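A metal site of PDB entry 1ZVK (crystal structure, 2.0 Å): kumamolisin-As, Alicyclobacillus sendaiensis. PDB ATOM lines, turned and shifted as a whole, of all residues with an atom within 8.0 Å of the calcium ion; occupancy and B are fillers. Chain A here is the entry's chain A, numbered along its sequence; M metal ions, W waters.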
ATOM      1  N   VAL A 207     -22.105 -11.607   7.897  1.00  0.00           N
ATOM      2  CA  VAL A 207     -21.370 -10.613   7.119  1.00  0.00           C
ATOM      3  C   VAL A 207     -20.087 -11.198   6.557  1.00  0.00           C
ATOM      4  O   VAL A 207     -19.386 -11.899   7.273  1.00  0.00           O
ATOM      5  CB  VAL A 207     -20.995  -9.358   7.933  1.00  0.00           C
ATOM      6  CG1 VAL A 207     -20.226  -8.359   7.079  1.00  0.00           C
ATOM      7  CG2 VAL A 207     -22.237  -8.699   8.534  1.00  0.00           C
ATOM      8  N   HIS A 315     -34.006 -11.840   3.497  1.00  0.00           N
ATOM      9  CA  HIS A 315     -33.396 -12.634   4.553  1.00  0.00           C
ATOM     10  C   HIS A 315     -32.515 -11.661   5.335  1.00  0.00           C
ATOM     11  O   HIS A 315     -31.456 -11.360   4.799  1.00  0.00           O
ATOM     12  CB  HIS A 315     -32.523 -13.808   4.110  1.00  0.00           C
ATOM     13  CG  HIS A 315     -31.984 -14.579   5.264  1.00  0.00           C
ATOM     14  ND1 HIS A 315     -30.682 -15.006   5.338  1.00  0.00           N
ATOM     15  CD2 HIS A 315     -32.585 -14.983   6.428  1.00  0.00           C
ATOM     16  CE1 HIS A 315     -30.489 -15.654   6.476  1.00  0.00           C
ATOM     17  NE2 HIS A 315     -31.626 -15.654   7.151  1.00  0.00           N
ATOM     18  N   ASP A 316     -32.935 -11.196   6.488  1.00  0.00           N
ATOM     19  CA  ASP A 316     -32.162 -10.215   7.222  1.00  0.00           C
ATOM     20  C   ASP A 316     -30.827 -10.765   7.670  1.00  0.00           C
ATOM     21  O   ASP A 316     -30.768 -11.863   8.212  1.00  0.00           O
ATOM     22  CB  ASP A 316     -32.946  -9.757   8.472  1.00  0.00           C
ATOM     23  CG  ASP A 316     -32.427  -8.537   9.201  1.00  0.00           C
ATOM     24  OD1 ASP A 316     -31.408  -7.924   8.850  1.00  0.00           O
ATOM     25  OD2 ASP A 316     -33.046  -8.065  10.184  1.00  0.00           O
ATOM     26  N   ILE A 317     -29.724 -10.028   7.481  1.00  0.00           N
ATOM     27  CA  ILE A 317     -28.473 -10.526   8.053  1.00  0.00           C
ATOM     28  C   ILE A 317     -28.219  -9.769   9.342  1.00  0.00           C
ATOM     29  O   ILE A 317     -28.305  -8.522   9.270  1.00  0.00           O
ATOM     30  CB  ILE A 317     -27.276 -10.338   7.117  1.00  0.00           C
ATOM     31  CG1 ILE A 317     -27.126 -11.403   6.043  1.00  0.00           C
ATOM     32  CG2 ILE A 317     -26.022 -10.247   7.993  1.00  0.00           C
ATOM     33  CD1 ILE A 317     -27.927 -11.206   4.786  1.00  0.00           C
ATOM     34  N   THR A 318     -27.937 -10.445  10.449  1.00  0.00           N
ATOM     35  CA  THR A 318     -27.789  -9.681  11.673  1.00  0.00           C
ATOM     36  C   THR A 318     -26.461  -9.901  12.358  1.00  0.00           C
ATOM     37  O   THR A 318     -26.111  -9.241  13.346  1.00  0.00           O
ATOM     38  CB  THR A 318     -28.915 -10.011  12.692  1.00  0.00           C
ATOM     39  OG1 THR A 318     -28.865 -11.414  12.940  1.00  0.00           O
ATOM     40  CG2 THR A 318     -30.293  -9.687  12.135  1.00  0.00           C
ATOM     41  N   GLU A 319     -25.649 -10.839  11.872  1.00  0.00           N
ATOM     42  CA  GLU A 319     -24.379 -10.997  12.568  1.00  0.00           C
ATOM     43  C   GLU A 319     -23.150 -10.727  11.693  1.00  0.00           C
ATOM     44  O   GLU A 319     -23.115 -10.988  10.484  1.00  0.00           O
ATOM     45  CB  GLU A 319     -24.276 -12.411  13.148  1.00  0.00           C
ATOM     46  CG  GLU A 319     -25.188 -12.663  14.328  1.00  0.00           C
ATOM     47  CD  GLU A 319     -25.590 -14.115  14.467  1.00  0.00           C
ATOM     48  OE1 GLU A 319     -24.713 -14.986  14.294  1.00  0.00           O
ATOM     49  OE2 GLU A 319     -26.783 -14.375  14.751  1.00  0.00           O
ATOM     50  N   GLN A 332     -21.201  -2.804  11.889  1.00  0.00           N
ATOM     51  CA  GLN A 332     -21.755  -4.085  12.322  1.00  0.00           C
ATOM     52  C   GLN A 332     -23.165  -4.361  11.832  1.00  0.00           C
ATOM     53  O   GLN A 332     -23.974  -3.464  11.593  1.00  0.00           O
ATOM     54  CB  GLN A 332     -21.683  -4.116  13.860  1.00  0.00           C
ATOM     55  CG  GLN A 332     -22.930  -4.644  14.532  1.00  0.00           C
ATOM     56  CD  GLN A 332     -23.011  -4.238  16.002  1.00  0.00           C
ATOM     57  OE1 GLN A 332     -23.985  -4.557  16.682  1.00  0.00           O
ATOM     58  NE2 GLN A 332     -21.974  -3.529  16.464  1.00  0.00           N
ATOM     59  N   ALA A 333     -23.484  -5.648  11.661  1.00  0.00           N
ATOM     60  CA  ALA A 333     -24.814  -6.046  11.212  1.00  0.00           C
ATOM     61  C   ALA A 333     -25.829  -5.956  12.355  1.00  0.00           C
ATOM     62  O   ALA A 333     -25.461  -5.797  13.507  1.00  0.00           O
ATOM     63  CB  ALA A 333     -24.791  -7.467  10.665  1.00  0.00           C
ATOM     64  N   GLY A 334     -27.118  -6.078  12.042  1.00  0.00           N
ATOM     65  CA  GLY A 334     -28.186  -6.110  13.035  1.00  0.00           C
ATOM     66  C   GLY A 334     -29.556  -6.193  12.403  1.00  0.00           C
ATOM     67  O   GLY A 334     -29.726  -6.277  11.188  1.00  0.00           O
ATOM     68  N   PRO A 335     -30.601  -6.183  13.227  1.00  0.00           N
ATOM     69  CA  PRO A 335     -31.962  -6.169  12.692  1.00  0.00           C
ATOM     70  C   PRO A 335     -32.176  -5.032  11.706  1.00  0.00           C
ATOM     71  O   PRO A 335     -31.784  -3.891  11.901  1.00  0.00           O
ATOM     72  CB  PRO A 335     -32.770  -5.930  13.969  1.00  0.00           C
ATOM     73  CG  PRO A 335     -31.985  -6.655  15.029  1.00  0.00           C
ATOM     74  CD  PRO A 335     -30.577  -6.205  14.697  1.00  0.00           C
ATOM     75  N   GLY A 336     -32.826  -5.340  10.595  1.00  0.00           N
ATOM     76  CA  GLY A 336     -33.119  -4.408   9.534  1.00  0.00           C
ATOM     77  C   GLY A 336     -31.868  -4.012   8.769  1.00  0.00           C
ATOM     78  O   GLY A 336     -30.840  -4.676   8.683  1.00  0.00           O
ATOM     79  N   TRP A 337     -32.012  -2.828   8.150  1.00  0.00           N
ATOM     80  CA  TRP A 337     -30.950  -2.271   7.334  1.00  0.00           C
ATOM     81  C   TRP A 337     -29.669  -2.126   8.137  1.00  0.00           C
ATOM     82  O   TRP A 337     -29.709  -1.586   9.256  1.00  0.00           O
ATOM     83  CB  TRP A 337     -31.371  -0.897   6.737  1.00  0.00           C
ATOM     84  CG  TRP A 337     -30.366  -0.443   5.717  1.00  0.00           C
ATOM     85  CD1 TRP A 337     -30.463  -0.638   4.366  1.00  0.00           C
ATOM     86  CD2 TRP A 337     -29.133   0.253   5.926  1.00  0.00           C
ATOM     87  NE1 TRP A 337     -29.378  -0.100   3.713  1.00  0.00           N
ATOM     88  CE2 TRP A 337     -28.535   0.447   4.653  1.00  0.00           C
ATOM     89  CE3 TRP A 337     -28.455   0.725   7.052  1.00  0.00           C
ATOM     90  CZ2 TRP A 337     -27.318   1.104   4.498  1.00  0.00           C
ATOM     91  CZ3 TRP A 337     -27.246   1.376   6.919  1.00  0.00           C
ATOM     92  CH2 TRP A 337     -26.697   1.546   5.628  1.00  0.00           C
ATOM     93  N   ASP A 338     -28.514  -2.559   7.606  1.00  0.00           N
ATOM     94  CA  ASP A 338     -27.280  -2.200   8.309  1.00  0.00           C
ATOM     95  C   ASP A 338     -26.202  -1.822   7.292  1.00  0.00           C
ATOM     96  O   ASP A 338     -26.325  -2.158   6.108  1.00  0.00           O
ATOM     97  CB  ASP A 338     -26.791  -3.316   9.229  1.00  0.00           C
ATOM     98  CG  ASP A 338     -26.670  -4.650   8.490  1.00  0.00           C
ATOM     99  OD1 ASP A 338     -25.806  -4.812   7.606  1.00  0.00           O
ATOM    100  OD2 ASP A 338     -27.512  -5.452   8.920  1.00  0.00           O
ATOM    101  N   PRO A 339     -25.146  -1.144   7.695  1.00  0.00           N
ATOM    102  CA  PRO A 339     -24.137  -0.731   6.718  1.00  0.00           C
ATOM    103  C   PRO A 339     -23.194  -1.846   6.284  1.00  0.00           C
ATOM    104  O   PRO A 339     -22.090  -1.592   5.763  1.00  0.00           O
ATOM    105  CB  PRO A 339     -23.342   0.358   7.463  1.00  0.00           C
ATOM    106  CG  PRO A 339     -23.916   0.487   8.826  1.00  0.00           C
ATOM    107  CD  PRO A 339     -24.812  -0.701   9.058  1.00  0.00           C
ATOM    108  N   CYS A 340     -23.570  -3.097   6.466  1.00  0.00           N
ATOM    109  CA  CYS A 340     -22.792  -4.247   5.989  1.00  0.00           C
ATOM    110  C   CYS A 340     -23.534  -4.963   4.861  1.00  0.00           C
ATOM    111  O   CYS A 340     -22.957  -5.304   3.824  1.00  0.00           O
ATOM    112  CB  CYS A 340     -22.514  -5.284   7.086  1.00  0.00           C
ATOM    113  SG  CYS A 340     -21.497  -4.683   8.458  1.00  0.00           S
ATOM    114  N   THR A 341     -24.824  -5.180   5.097  1.00  0.00           N
ATOM    115  CA  THR A 341     -25.665  -5.965   4.202  1.00  0.00           C
ATOM    116  C   THR A 341     -26.931  -5.278   3.772  1.00  0.00           C
ATOM    117  O   THR A 341     -27.790  -5.814   3.075  1.00  0.00           O
ATOM    118  CB  THR A 341     -26.027  -7.260   4.956  1.00  0.00           C
ATOM    119  OG1 THR A 341     -26.629  -6.944   6.219  1.00  0.00           O
ATOM    120  CG2 THR A 341     -24.723  -8.019   5.196  1.00  0.00           C
ATOM    121  N   GLY A 342     -27.125  -4.033   4.180  1.00  0.00           N
ATOM    122  CA  GLY A 342     -28.282  -3.277   3.748  1.00  0.00           C
ATOM    123  C   GLY A 342     -29.581  -3.918   4.170  1.00  0.00           C
ATOM    124  O   GLY A 342     -29.751  -4.266   5.322  1.00  0.00           O
ATOM    125  N   LEU A 343     -30.503  -4.058   3.205  1.00  0.00           N
ATOM    126  CA  LEU A 343     -31.782  -4.659   3.547  1.00  0.00           C
ATOM    127  C   LEU A 343     -31.625  -6.161   3.724  1.00  0.00           C
ATOM    128  O   LEU A 343     -32.573  -6.727   4.255  1.00  0.00           O
ATOM    129  CB  LEU A 343     -32.810  -4.347   2.481  1.00  0.00           C
ATOM    130  CG  LEU A 343     -33.162  -2.850   2.331  1.00  0.00           C
ATOM    131  CD1 LEU A 343     -33.984  -2.655   1.053  1.00  0.00           C
ATOM    132  CD2 LEU A 343     -33.881  -2.328   3.553  1.00  0.00           C
ATOM    133  N   GLY A 344     -30.492  -6.744   3.312  1.00  0.00           N
ATOM    134  CA  GLY A 344     -30.276  -8.188   3.467  1.00  0.00           C
ATOM    135  C   GLY A 344     -30.198  -8.866   2.108  1.00  0.00           C
ATOM    136  O   GLY A 344     -29.922  -8.188   1.107  1.00  0.00           O
ATOM    137  N   SER A 345     -30.457 -10.186   2.077  1.00  0.00           N
ATOM    138  CA  SER A 345     -30.502 -10.872   0.785  1.00  0.00           C
ATOM    139  C   SER A 345     -31.956 -10.936   0.307  1.00  0.00           C
ATOM    140  O   SER A 345     -32.858 -11.227   1.110  1.00  0.00           O
ATOM    141  CB  SER A 345     -29.935 -12.298   0.770  1.00  0.00           C
ATOM    142  OG  SER A 345     -30.533 -13.174   1.713  1.00  0.00           O
HETATM  143 CA    CA M   1     -29.562  -6.577   8.901  1.00  0.00          CA
HETATM  144  O   HOH W   1     -29.263  -6.796   6.599  1.00  0.00           O
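The side-chain carboxylate (OD1) of Asp 316 binds the calcium ion, 2.3 Å away.
O of Gly 336 binds the calcium ion.
The backbone carbonyl oxygen (O) of Gly 334 is bound to the calcium ion.
Water W1 is bound to the calcium ion (2.3 Å).
OD2 of Asp 338 is bound to the calcium ion (2.3 Å).
The calcium ion is bound by O of Ile 317, at 2.3 Å.
Water W1 lies within hydrogen-bond range of the side-chain hydroxyl of Thr 341, the backbone carbonyl oxygen of Gly 342 and the backbone NH of Ile 317.
The side-chain carboxylate (OD1) of Asp 338 is in hydrogen-bond range of the side-chain hydroxyl (OG1) of Thr 341 (2.7 Å).
The side-chain carboxylate (OD1) of Asp 338 sits close to the backbone NH (N) of Cys 340, at 3.0 Å.
OG1 of Thr 341 touches the calcium ion (3.99 Å).
Within 4 Å of the calcium ion: Asp 316, Ile 317, Gly 334, Gly 336, Asp 338 and Thr 341.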
